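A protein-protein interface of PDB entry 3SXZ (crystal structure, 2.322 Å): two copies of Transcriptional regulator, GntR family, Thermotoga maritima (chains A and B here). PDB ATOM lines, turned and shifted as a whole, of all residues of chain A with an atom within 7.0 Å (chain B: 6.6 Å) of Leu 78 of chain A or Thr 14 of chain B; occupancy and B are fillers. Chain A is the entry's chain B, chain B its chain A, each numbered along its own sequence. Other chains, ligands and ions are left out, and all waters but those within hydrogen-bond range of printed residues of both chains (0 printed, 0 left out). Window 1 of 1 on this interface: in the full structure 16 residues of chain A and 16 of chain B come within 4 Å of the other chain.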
ATOM      1  N   THR A  14      18.994   2.889   2.457  1.00  0.00           N
ATOM      2  CA  THR A  14      17.915   3.800   2.845  1.00  0.00           C
ATOM      3  C   THR A  14      17.815   4.930   1.819  1.00  0.00           C
ATOM      4  O   THR A  14      16.726   5.315   1.415  1.00  0.00           O
ATOM      5  CB  THR A  14      18.129   4.392   4.263  1.00  0.00           C
ATOM      6  OG1 THR A  14      18.167   3.337   5.230  1.00  0.00           O
ATOM      7  CG2 THR A  14      17.002   5.351   4.631  1.00  0.00           C
ATOM      8  N   MET A  17      16.179   3.601  -1.327  1.00  0.00           N
ATOM      9  CA  MET A  17      14.743   3.475  -1.111  1.00  0.00           C
ATOM     10  C   MET A  17      14.035   4.817  -1.292  1.00  0.00           C
ATOM     11  O   MET A  17      13.026   4.908  -1.991  1.00  0.00           O
ATOM     12  CB  MET A  17      14.474   2.926   0.300  1.00  0.00           C
ATOM     13  CG  MET A  17      13.014   2.991   0.734  1.00  0.00           C
ATOM     14  SD  MET A  17      12.717   2.474   2.449  1.00  0.00           S
ATOM     15  CE  MET A  17      13.376   3.873   3.348  1.00  0.00           C
ATOM     16  N   MET A  18      14.570   5.864  -0.679  1.00  0.00           N
ATOM     17  CA  MET A  18      13.864   7.137  -0.630  1.00  0.00           C
ATOM     18  C   MET A  18      14.047   7.965  -1.892  1.00  0.00           C
ATOM     19  O   MET A  18      13.101   8.564  -2.400  1.00  0.00           O
ATOM     20  CB  MET A  18      14.335   7.947   0.583  1.00  0.00           C
ATOM     21  CG  MET A  18      13.995   7.305   1.916  1.00  0.00           C
ATOM     22  SD  MET A  18      14.590   8.238   3.332  1.00  0.00           S
ATOM     23  CE  MET A  18      13.442   9.602   3.373  1.00  0.00           C
ATOM     24  N   PHE A  21      12.497   6.303  -5.092  1.00  0.00           N
ATOM     25  CA  PHE A  21      11.053   6.473  -5.004  1.00  0.00           C
ATOM     26  C   PHE A  21      10.654   7.880  -5.439  1.00  0.00           C
ATOM     27  O   PHE A  21       9.719   8.057  -6.210  1.00  0.00           O
ATOM     28  CB  PHE A  21      10.541   6.210  -3.589  1.00  0.00           C
ATOM     29  CG  PHE A  21       9.054   6.379  -3.452  1.00  0.00           C
ATOM     30  CD1 PHE A  21       8.200   5.329  -3.719  1.00  0.00           C
ATOM     31  CD2 PHE A  21       8.511   7.595  -3.080  1.00  0.00           C
ATOM     32  CE1 PHE A  21       6.830   5.477  -3.604  1.00  0.00           C
ATOM     33  CE2 PHE A  21       7.139   7.750  -2.963  1.00  0.00           C
ATOM     34  CZ  PHE A  21       6.300   6.681  -3.229  1.00  0.00           C
ATOM     35  N   ILE A  67      14.232  14.529  -3.110  1.00  0.00           N
ATOM     36  CA  ILE A  67      13.350  14.281  -1.976  1.00  0.00           C
ATOM     37  C   ILE A  67      12.298  15.384  -1.825  1.00  0.00           C
ATOM     38  O   ILE A  67      11.106  15.116  -1.637  1.00  0.00           O
ATOM     39  CB  ILE A  67      14.178  14.188  -0.674  1.00  0.00           C
ATOM     40  CG1 ILE A  67      15.162  13.004  -0.735  1.00  0.00           C
ATOM     41  CG2 ILE A  67      13.267  14.076   0.512  1.00  0.00           C
ATOM     42  CD1 ILE A  67      14.522  11.635  -0.818  1.00  0.00           C
ATOM     43  N   ASN A  72       6.231  16.022   0.023  1.00  0.00           N
ATOM     44  CA  ASN A  72       5.800  15.226   1.171  1.00  0.00           C
ATOM     45  C   ASN A  72       6.644  15.524   2.413  1.00  0.00           C
ATOM     46  O   ASN A  72       7.792  15.094   2.523  1.00  0.00           O
ATOM     47  CB  ASN A  72       5.865  13.742   0.821  1.00  0.00           C
ATOM     48  CG  ASN A  72       5.361  12.852   1.938  1.00  0.00           C
ATOM     49  OD1 ASN A  72       5.539  13.134   3.126  1.00  0.00           O
ATOM     50  ND2 ASN A  72       4.724  11.766   1.553  1.00  0.00           N
ATOM     51  N   GLU A  73       6.041  16.219   3.348  1.00  0.00           N
ATOM     52  CA  GLU A  73       6.727  16.712   4.504  1.00  0.00           C
ATOM     53  C   GLU A  73       7.267  15.649   5.424  1.00  0.00           C
ATOM     54  O   GLU A  73       8.288  15.825   6.032  1.00  0.00           O
ATOM     55  CB  GLU A  73       5.836  17.673   5.247  1.00  0.00           C
ATOM     56  CG  GLU A  73       5.444  18.804   4.383  1.00  0.00           C
ATOM     57  CD  GLU A  73       6.278  20.013   4.597  1.00  0.00           C
ATOM     58  OE1 GLU A  73       5.748  20.950   5.209  1.00  0.00           O
ATOM     59  OE2 GLU A  73       7.444  20.041   4.177  1.00  0.00           O
ATOM     60  N   LEU A  74       6.552  14.554   5.520  1.00  0.00           N
ATOM     61  CA  LEU A  74       7.017  13.426   6.318  1.00  0.00           C
ATOM     62  C   LEU A  74       8.286  12.836   5.704  1.00  0.00           C
ATOM     63  O   LEU A  74       9.284  12.649   6.384  1.00  0.00           O
ATOM     64  CB  LEU A  74       5.938  12.346   6.434  1.00  0.00           C
ATOM     65  CG  LEU A  74       6.300  11.149   7.315  1.00  0.00           C
ATOM     66  CD1 LEU A  74       6.670  11.610   8.730  1.00  0.00           C
ATOM     67  CD2 LEU A  74       5.150  10.140   7.372  1.00  0.00           C
ATOM     68  N   ILE A  75       8.251  12.561   4.410  1.00  0.00           N
ATOM     69  CA  ILE A  75       9.414  12.010   3.721  1.00  0.00           C
ATOM     70  C   ILE A  75      10.593  12.985   3.791  1.00  0.00           C
ATOM     71  O   ILE A  75      11.731  12.581   4.027  1.00  0.00           O
ATOM     72  CB  ILE A  75       9.089  11.703   2.255  1.00  0.00           C
ATOM     73  CG1 ILE A  75       8.078  10.555   2.184  1.00  0.00           C
ATOM     74  CG2 ILE A  75      10.367  11.382   1.479  1.00  0.00           C
ATOM     75  CD1 ILE A  75       7.653  10.169   0.791  1.00  0.00           C
ATOM     76  N   ILE A  76      10.312  14.272   3.594  1.00  0.00           N
ATOM     77  CA  ILE A  76      11.344  15.300   3.654  1.00  0.00           C
ATOM     78  C   ILE A  76      12.017  15.319   5.032  1.00  0.00           C
ATOM     79  O   ILE A  76      13.245  15.368   5.132  1.00  0.00           O
ATOM     80  CB  ILE A  76      10.764  16.682   3.339  1.00  0.00           C
ATOM     81  CG1 ILE A  76      10.418  16.767   1.849  1.00  0.00           C
ATOM     82  CG2 ILE A  76      11.764  17.786   3.730  1.00  0.00           C
ATOM     83  CD1 ILE A  76       9.489  17.913   1.465  1.00  0.00           C
ATOM     84  N   SER A  77      11.222  15.261   6.096  1.00  0.00           N
ATOM     85  CA  SER A  77      11.784  15.327   7.437  1.00  0.00           C
ATOM     86  C   SER A  77      12.504  14.028   7.822  1.00  0.00           C
ATOM     87  O   SER A  77      13.481  14.066   8.561  1.00  0.00           O
ATOM     88  CB  SER A  77      10.725  15.732   8.472  1.00  0.00           C
ATOM     89  OG  SER A  77       9.764  14.722   8.712  1.00  0.00           O
ATOM     90  N   LEU A  78      12.067  12.893   7.287  1.00  0.00           N
ATOM     91  CA  LEU A  78      12.773  11.641   7.534  1.00  0.00           C
ATOM     92  C   LEU A  78      14.158  11.696   6.889  1.00  0.00           C
ATOM     93  O   LEU A  78      15.135  11.222   7.455  1.00  0.00           O
ATOM     94  CB  LEU A  78      11.992  10.438   7.000  1.00  0.00           C
ATOM     95  CG  LEU A  78      10.679  10.024   7.683  1.00  0.00           C
ATOM     96  CD1 LEU A  78      10.101   8.825   6.954  1.00  0.00           C
ATOM     97  CD2 LEU A  78      10.824   9.703   9.167  1.00  0.00           C
ATOM     98  N   TYR A  79      14.246  12.288   5.706  1.00  0.00           N
ATOM     99  CA  TYR A  79      15.528  12.395   5.022  1.00  0.00           C
ATOM    100  C   TYR A  79      16.444  13.354   5.775  1.00  0.00           C
ATOM    101  O   TYR A  79      17.657  13.146   5.852  1.00  0.00           O
ATOM    102  CB  TYR A  79      15.325  12.891   3.600  1.00  0.00           C
ATOM    103  CG  TYR A  79      16.532  12.687   2.724  1.00  0.00           C
ATOM    104  CD1 TYR A  79      16.828  11.432   2.207  1.00  0.00           C
ATOM    105  CD2 TYR A  79      17.373  13.748   2.403  1.00  0.00           C
ATOM    106  CE1 TYR A  79      17.936  11.237   1.399  1.00  0.00           C
ATOM    107  CE2 TYR A  79      18.477  13.561   1.594  1.00  0.00           C
ATOM    108  CZ  TYR A  79      18.753  12.301   1.100  1.00  0.00           C
ATOM    109  OH  TYR A  79      19.842  12.106   0.295  1.00  0.00           O
ATOM    110  N   GLU A  80      15.849  14.409   6.327  1.00  0.00           N
ATOM    111  CA  GLU A  80      16.588  15.390   7.113  1.00  0.00           C
ATOM    112  C   GLU A  80      17.121  14.736   8.386  1.00  0.00           C
ATOM    113  O   GLU A  80      18.240  15.018   8.824  1.00  0.00           O
ATOM    114  CB  GLU A  80      15.685  16.575   7.469  1.00  0.00           C
ATOM    115  CG  GLU A  80      16.440  17.838   7.814  1.00  0.00           C
ATOM    116  CD  GLU A  80      17.270  18.337   6.651  1.00  0.00           C
ATOM    117  OE1 GLU A  80      16.728  18.396   5.521  1.00  0.00           O
ATOM    118  OE2 GLU A  80      18.464  18.652   6.863  1.00  0.00           O
ATOM    119  N   LYS A  81      16.321  13.843   8.961  1.00  0.00           N
ATOM    120  CA  LYS A  81      16.688  13.140  10.189  1.00  0.00           C
ATOM    121  C   LYS A  81      17.968  12.340   9.997  1.00  0.00           C
ATOM    122  O   LYS A  81      18.805  12.259  10.905  1.00  0.00           O
ATOM    123  CB  LYS A  81      15.552  12.211  10.633  1.00  0.00           C
ATOM    124  CG  LYS A  81      15.835  11.419  11.905  1.00  0.00           C
ATOM    125  CD  LYS A  81      14.936  11.857  13.046  1.00  0.00           C
ATOM    126  CE  LYS A  81      15.498  11.429  14.395  1.00  0.00           C
ATOM    127  NZ  LYS A  81      15.461  12.551  15.371  1.00  0.00           N
ATOM    128  N   ILE A  82      18.130  11.773   8.805  1.00  0.00           N
ATOM    129  CA  ILE A  82      19.273  10.909   8.531  1.00  0.00           C
ATOM    130  C   ILE A  82      20.380  11.606   7.746  1.00  0.00           C
ATOM    131  O   ILE A  82      21.386  10.982   7.428  1.00  0.00           O
ATOM    132  CB  ILE A  82      18.849   9.623   7.791  1.00  0.00           C
ATOM    133  CG1 ILE A  82      18.341   9.936   6.383  1.00  0.00           C
ATOM    134  CG2 ILE A  82      17.788   8.907   8.601  1.00  0.00           C
ATOM    135  CD1 ILE A  82      18.260   8.722   5.467  1.00  0.00           C
ATOM    136  N   TRP A  83      20.218  12.893   7.452  1.00  0.00           N
ATOM    137  CA  TRP A  83      21.217  13.593   6.654  1.00  0.00           C
ATOM    138  C   TRP A  83      22.621  13.581   7.275  1.00  0.00           C
ATOM    139  O   TRP A  83      23.607  13.372   6.574  1.00  0.00           O
ATOM    140  CB  TRP A  83      20.834  15.043   6.347  1.00  0.00           C
ATOM    141  CG  TRP A  83      21.964  15.662   5.621  1.00  0.00           C
ATOM    142  CD1 TRP A  83      22.875  16.556   6.113  1.00  0.00           C
ATOM    143  CD2 TRP A  83      22.368  15.371   4.277  1.00  0.00           C
ATOM    144  NE1 TRP A  83      23.809  16.852   5.148  1.00  0.00           N
ATOM    145  CE2 TRP A  83      23.519  16.140   4.014  1.00  0.00           C
ATOM    146  CE3 TRP A  83      21.865  14.539   3.273  1.00  0.00           C
ATOM    147  CZ2 TRP A  83      24.168  16.105   2.786  1.00  0.00           C
ATOM    148  CZ3 TRP A  83      22.508  14.509   2.052  1.00  0.00           C
ATOM    149  CH2 TRP A  83      23.648  15.286   1.819  1.00  0.00           C
ATOM    150  N   ARG B   9      -2.543  11.488   3.331  1.00  0.00           N
ATOM    151  CA  ARG B   9      -1.909  11.155   2.080  1.00  0.00           C
ATOM    152  C   ARG B   9      -0.412  10.978   2.213  1.00  0.00           C
ATOM    153  O   ARG B   9       0.132  10.082   1.660  1.00  0.00           O
ATOM    154  CB  ARG B   9      -2.234  12.165   0.987  1.00  0.00           C
ATOM    155  CG  ARG B   9      -3.694  12.225   0.614  1.00  0.00           C
ATOM    156  CD  ARG B   9      -4.009  12.974  -0.668  1.00  0.00           C
ATOM    157  NE  ARG B   9      -3.258  14.202  -0.789  1.00  0.00           N
ATOM    158  CZ  ARG B   9      -3.711  15.413  -0.503  1.00  0.00           C
ATOM    159  NH1 ARG B   9      -4.952  15.611  -0.074  1.00  0.00           N
ATOM    160  NH2 ARG B   9      -2.900  16.432  -0.633  1.00  0.00           N
ATOM    161  N   GLU B  10       0.232  11.846   2.955  1.00  0.00           N
ATOM    162  CA  GLU B  10       1.665  11.768   3.182  1.00  0.00           C
ATOM    163  C   GLU B  10       2.026  10.507   3.940  1.00  0.00           C
ATOM    164  O   GLU B  10       3.060   9.902   3.680  1.00  0.00           O
ATOM    165  CB  GLU B  10       2.144  12.975   3.969  1.00  0.00           C
ATOM    166  CG  GLU B  10       2.195  14.246   3.166  1.00  0.00           C
ATOM    167  CD  GLU B  10       2.712  15.402   3.986  1.00  0.00           C
ATOM    168  OE1 GLU B  10       2.711  15.289   5.232  1.00  0.00           O
ATOM    169  OE2 GLU B  10       3.123  16.419   3.387  1.00  0.00           O
ATOM    170  N   THR B  11       1.164  10.115   4.872  1.00  0.00           N
ATOM    171  CA  THR B  11       1.413   8.933   5.686  1.00  0.00           C
ATOM    172  C   THR B  11       1.406   7.726   4.769  1.00  0.00           C
ATOM    173  O   THR B  11       2.331   6.921   4.783  1.00  0.00           O
ATOM    174  CB  THR B  11       0.341   8.722   6.782  1.00  0.00           C
ATOM    175  OG1 THR B  11       0.246   9.882   7.614  1.00  0.00           O
ATOM    176  CG2 THR B  11       0.707   7.534   7.662  1.00  0.00           C
ATOM    177  N   ILE B  12       0.362   7.626   3.956  1.00  0.00           N
ATOM    178  CA  ILE B  12       0.177   6.478   3.088  1.00  0.00           C
ATOM    179  C   ILE B  12       1.269   6.399   2.026  1.00  0.00           C
ATOM    180  O   ILE B  12       1.767   5.316   1.738  1.00  0.00           O
ATOM    181  CB  ILE B  12      -1.204   6.510   2.413  1.00  0.00           C
ATOM    182  CG1 ILE B  12      -2.311   6.414   3.485  1.00  0.00           C
ATOM    183  CG2 ILE B  12      -1.266   5.407   1.352  1.00  0.00           C
ATOM    184  CD1 ILE B  12      -2.377   5.099   4.254  1.00  0.00           C
ATOM    185  N   GLU B  13       1.647   7.540   1.458  1.00  0.00           N
ATOM    186  CA  GLU B  13       2.732   7.577   0.488  1.00  0.00           C
ATOM    187  C   GLU B  13       4.049   7.116   1.112  1.00  0.00           C
ATOM    188  O   GLU B  13       4.830   6.434   0.463  1.00  0.00           O
ATOM    189  CB  GLU B  13       2.899   8.974  -0.106  1.00  0.00           C
ATOM    190  CG  GLU B  13       3.993   9.033  -1.155  1.00  0.00           C
ATOM    191  CD  GLU B  13       4.079  10.367  -1.871  1.00  0.00           C
ATOM    192  OE1 GLU B  13       3.872  11.413  -1.224  1.00  0.00           O
ATOM    193  OE2 GLU B  13       4.354  10.368  -3.090  1.00  0.00           O
ATOM    194  N   THR B  14       4.279   7.472   2.371  1.00  0.00           N
ATOM    195  CA  THR B  14       5.502   7.073   3.060  1.00  0.00           C
ATOM    196  C   THR B  14       5.478   5.561   3.270  1.00  0.00           C
ATOM    197  O   THR B  14       6.491   4.886   3.100  1.00  0.00           O
ATOM    198  CB  THR B  14       5.675   7.805   4.418  1.00  0.00           C
ATOM    199  OG1 THR B  14       5.739   9.217   4.193  1.00  0.00           O
ATOM    200  CG2 THR B  14       6.953   7.364   5.134  1.00  0.00           C
ATOM    201  N   ARG B  15       4.316   5.031   3.634  1.00  0.00           N
ATOM    202  CA  ARG B  15       4.177   3.598   3.847  1.00  0.00           C
ATOM    203  C   ARG B  15       4.384   2.845   2.539  1.00  0.00           C
ATOM    204  O   ARG B  15       4.987   1.775   2.519  1.00  0.00           O
ATOM    205  CB  ARG B  15       2.795   3.266   4.391  1.00  0.00           C
ATOM    206  CG  ARG B  15       2.534   3.717   5.822  1.00  0.00           C
ATOM    207  CD  ARG B  15       1.171   3.209   6.268  1.00  0.00           C
ATOM    208  NE  ARG B  15       1.215   1.770   6.479  1.00  0.00           N
ATOM    209  CZ  ARG B  15       0.167   1.017   6.778  1.00  0.00           C
ATOM    210  NH1 ARG B  15      -1.036   1.560   6.914  1.00  0.00           N
ATOM    211  NH2 ARG B  15       0.330  -0.289   6.941  1.00  0.00           N
ATOM    212  N   ILE B  16       3.873   3.398   1.447  1.00  0.00           N
ATOM    213  CA  ILE B  16       4.033   2.768   0.148  1.00  0.00           C
ATOM    214  C   ILE B  16       5.517   2.716  -0.197  1.00  0.00           C
ATOM    215  O   ILE B  16       6.036   1.674  -0.591  1.00  0.00           O
ATOM    216  CB  ILE B  16       3.235   3.501  -0.952  1.00  0.00           C
ATOM    217  CG1 ILE B  16       1.740   3.178  -0.814  1.00  0.00           C
ATOM    218  CG2 ILE B  16       3.736   3.086  -2.350  1.00  0.00           C
ATOM    219  CD1 ILE B  16       0.821   3.971  -1.722  1.00  0.00           C
ATOM    220  N   MET B  17       6.203   3.836  -0.010  1.00  0.00           N
ATOM    221  CA  MET B  17       7.631   3.911  -0.290  1.00  0.00           C
ATOM    222  C   MET B  17       8.418   2.852   0.484  1.00  0.00           C
ATOM    223  O   MET B  17       9.271   2.168  -0.074  1.00  0.00           O
ATOM    224  CB  MET B  17       8.158   5.298   0.065  1.00  0.00           C
ATOM    225  CG  MET B  17       9.677   5.408   0.047  1.00  0.00           C
ATOM    226  SD  MET B  17      10.277   7.014   0.579  1.00  0.00           S
ATOM    227  CE  MET B  17      10.012   6.910   2.356  1.00  0.00           C
ATOM    228  N   MET B  18       8.131   2.711   1.772  1.00  0.00           N
ATOM    229  CA  MET B  18       8.970   1.875   2.627  1.00  0.00           C
ATOM    230  C   MET B  18       8.614   0.402   2.534  1.00  0.00           C
ATOM    231  O   MET B  18       9.488  -0.453   2.468  1.00  0.00           O
ATOM    232  CB  MET B  18       8.866   2.336   4.081  1.00  0.00           C
ATOM    233  CG  MET B  18       9.429   3.726   4.328  1.00  0.00           C
ATOM    234  SD  MET B  18       9.289   4.252   6.053  1.00  0.00           S
ATOM    235  CE  MET B  18      10.595   3.307   6.816  1.00  0.00           C
ATOM    236  N   GLU B  19       7.321   0.120   2.527  1.00  0.00           N
ATOM    237  CA  GLU B  19       6.829  -1.249   2.576  1.00  0.00           C
ATOM    238  C   GLU B  19       6.974  -1.963   1.242  1.00  0.00           C
ATOM    239  O   GLU B  19       7.317  -3.142   1.201  1.00  0.00           O
ATOM    240  CB  GLU B  19       5.365  -1.269   3.004  1.00  0.00           C
ATOM    241  CG  GLU B  19       5.126  -0.753   4.420  1.00  0.00           C
ATOM    242  CD  GLU B  19       3.707  -0.998   4.870  1.00  0.00           C
ATOM    243  OE1 GLU B  19       3.096  -1.961   4.367  1.00  0.00           O
ATOM    244  OE2 GLU B  19       3.192  -0.243   5.720  1.00  0.00           O
ATOM    245  N   LEU B  78      13.147   4.042  11.382  1.00  0.00           N
ATOM    246  CA  LEU B  78      12.387   5.107  10.743  1.00  0.00           C
ATOM    247  C   LEU B  78      10.905   4.722  10.733  1.00  0.00           C
ATOM    248  O   LEU B  78      10.035   5.555  10.977  1.00  0.00           O
ATOM    249  CB  LEU B  78      12.883   5.367   9.315  1.00  0.00           C
ATOM    250  CG  LEU B  78      14.261   6.021   9.113  1.00  0.00           C
ATOM    251  CD1 LEU B  78      14.531   6.160   7.631  1.00  0.00           C
ATOM    252  CD2 LEU B  78      14.415   7.370   9.807  1.00  0.00           C
ATOM    253  N   TYR B  79      10.619   3.452  10.477  1.00  0.00           N
ATOM    254  CA  TYR B  79       9.238   2.997  10.427  1.00  0.00           C
ATOM    255  C   TYR B  79       8.618   3.071  11.821  1.00  0.00           C
ATOM    256  O   TYR B  79       7.446   3.414  11.980  1.00  0.00           O
ATOM    257  CB  TYR B  79       9.167   1.571   9.901  1.00  0.00           C
ATOM    258  CG  TYR B  79       7.778   1.157   9.476  1.00  0.00           C
ATOM    259  CD1 TYR B  79       7.235   1.604   8.278  1.00  0.00           C
ATOM    260  CD2 TYR B  79       7.013   0.308  10.264  1.00  0.00           C
ATOM    261  CE1 TYR B  79       5.969   1.225   7.885  1.00  0.00           C
ATOM    262  CE2 TYR B  79       5.751  -0.073   9.878  1.00  0.00           C
ATOM    263  CZ  TYR B  79       5.232   0.395   8.692  1.00  0.00           C
ATOM    264  OH  TYR B  79       3.975   0.007   8.302  1.00  0.00           O
ATOM    265  N   LYS B  81       9.516   5.183  14.107  1.00  0.00           N
ATOM    266  CA  LYS B  81       9.350   6.606  14.389  1.00  0.00           C
ATOM    267  C   LYS B  81       7.978   7.106  13.923  1.00  0.00           C
ATOM    268  O   LYS B  81       7.373   7.971  14.550  1.00  0.00           O
ATOM    269  CB  LYS B  81      10.467   7.412  13.710  1.00  0.00           C
ATOM    270  CG  LYS B  81      10.385   8.914  13.929  1.00  0.00           C
ATOM    271  CD  LYS B  81      11.562   9.413  14.742  1.00  0.00           C
ATOM    272  CE  LYS B  81      11.277  10.769  15.368  1.00  0.00           C
ATOM    273  NZ  LYS B  81      11.644  10.780  16.815  1.00  0.00           N
ATOM    274  N   ILE B  82       7.486   6.553  12.821  1.00  0.00           N
ATOM    275  CA  ILE B  82       6.234   7.028  12.252  1.00  0.00           C
ATOM    276  C   ILE B  82       5.060   6.104  12.552  1.00  0.00           C
ATOM    277  O   ILE B  82       3.949   6.355  12.096  1.00  0.00           O
ATOM    278  CB  ILE B  82       6.346   7.246  10.732  1.00  0.00           C
ATOM    279  CG1 ILE B  82       6.557   5.917   9.998  1.00  0.00           C
ATOM    280  CG2 ILE B  82       7.482   8.211  10.439  1.00  0.00           C
ATOM    281  CD1 ILE B  82       6.293   5.985   8.506  1.00  0.00           C
ATOM    282  N   ARG B  85       1.886   7.654  14.057  1.00  0.00           N
ATOM    283  CA  ARG B  85       1.201   8.397  13.009  1.00  0.00           C
ATOM    284  C   ARG B  85       0.422   7.445  12.098  1.00  0.00           C
ATOM    285  O   ARG B  85      -0.719   7.718  11.731  1.00  0.00           O
ATOM    286  CB  ARG B  85       2.213   9.212  12.209  1.00  0.00           C
ATOM    287  CG  ARG B  85       1.654   9.875  10.983  1.00  0.00           C
ATOM    288  CD  ARG B  85       2.541  11.031  10.557  1.00  0.00           C
ATOM    289  NE  ARG B  85       2.135  11.567   9.263  1.00  0.00           N
ATOM    290  CZ  ARG B  85       2.489  12.758   8.789  1.00  0.00           C
ATOM    291  NH1 ARG B  85       3.265  13.576   9.494  1.00  0.00           N
ATOM    292  NH2 ARG B  85       2.058  13.132   7.595  1.00  0.00           N
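The backbone carbonyl oxygen (O) of Glu 10 of chain B lies within hydrogen-bond range of the side-chain amide nitrogen (ND2) of Asn 72 of chain A (3.3 Å).
The side-chain carboxylate of Glu 10 of chain B is in hydrogen-bond range of the backbone NH of Glu 73 of chain A (2.9 Å).
OE1 of Glu 13 of chain B lies within hydrogen-bond range of ND2 of Asn 72 of chain A, 2.9 Å away.
The side-chain hydroxyl (OG1) of Thr 14 of chain B sits at hydrogen-bond distance from the backbone carbonyl oxygen (O) of Glu 10 of chain B (2.8 Å).
The side-chain hydroxyl (OG1) of Thr 11 of chain B is in hydrogen-bond range of the guanidinium group (NE) of Arg 85 of chain B, 3.0 Å away.
The backbone NH of Leu 74 of chain A lies within hydrogen-bond range of the side-chain amide oxygen of Asn 72 of chain A, at 3.0 Å.
The side-chain amide oxygen of Asn 72 of chain A sits at hydrogen-bond distance from the backbone NH of Ile 75 of chain A (3.1 Å).
The backbone carbonyl oxygen of Glu 73 of chain A lies within hydrogen-bond range of the side-chain hydroxyl of Ser 77 of chain A, at 3.3 Å.
O of Leu 74 of chain A is in hydrogen-bond range of OG of Ser 77 of chain A (3.2 Å).
Among the printed residues, merely in contact across the chains: Thr 14 of chain A with Leu 78 of chain B (3.97 Å), Met 17 of chain A with Met 17 of chain B (3.9 Å), Met 17 of chain A with Met 18 of chain B (3.8 Å), Met 18 of chain A with Met 17 of chain B (3.8 Å), Phe 21 of chain A with Glu 13 of chain B (3.8 Å), Phe 21 of chain A with Met 17 of chain B (3.7 Å), Asn 72 of chain A with Thr 14 of chain B (3.8 Å), Leu 74 of chain A with Glu 10 of chain B (3.9 Å), Leu 74 of chain A with Thr 14 of chain B (3.4 Å), Leu 74 of chain A with Ile 82 of chain B (3.9 Å), Leu 74 of chain A with Arg 85 of chain B (3.8 Å), Ile 75 of chain A with Thr 14 of chain B (3.4 Å), Leu 78 of chain A with Thr 14 of chain B (3.9 Å), Leu 78 of chain A with Ile 82 of chain B (3.9 Å) and Ile 82 of chain A with Leu 78 of chain B (3.9 Å).
Leu 78 of chain A touches two residues of chain B.
Arg 9 of chain B touches none of the printed residues of chain A.
Of the printed residues of chain A, Glu 10 of chain B touches Asn 72, Glu 73 and Leu 74.
Thr 14 of chain B touches four residues of chain A.
Of the printed residues of chain A, Leu 78 of chain B touches Thr 14 (3.97 Å) and Ile 82 (3.9 Å).
The nearest residue of chain B that does not touch Leu 78 of chain A is Leu 78 of chain B (4.3 Å).
The nearest printed residue of chain A that does not touch Met 17 of chain B is Ile 75 of chain A (4.1 Å).
Hydrophobic or aromatic side chains of chain A within 4 Å of the printed part of chain B: Met 17, Met 18, Phe 21, Leu 74, Ile 75, Leu 78 and Ile 82.
Along chain A the printed residues that touch a printed residue of chain B span positions 14 to 82.
Of the 16 printed residues of chain B, 8 touch a printed residue of chain A.
Hydrophobic or aromatic side chains of chain B that line the printed part of chain A: Met 17, Met 18, Leu 78 and Ile 82.
Among the printed residues, no Asp or Glu carboxylate lies within 4 Å of a Lys or Arg side-chain nitrogen of the other chain.
Thr 14 of chain A touches Leu 78 of chain B, and with the chains exchanged Leu 78 of chain A touches Thr 14 of chain B.
Met 17 of chain B touches its own counterpart, Met 17 of chain A.
Met 17 of chain A touches Met 18 of chain B, and with the chains exchanged Met 18 of chain A touches Met 17 of chain B.
Leu 78 of chain A touches Ile 82 of chain B, and with the chains exchanged Ile 82 of chain A touches Leu 78 of chain B.
7 positions are printed for both chains.
Of the 18 pairs that touch across the chains among the printed residues, 7 have their exchanged pair printed and touching as well.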
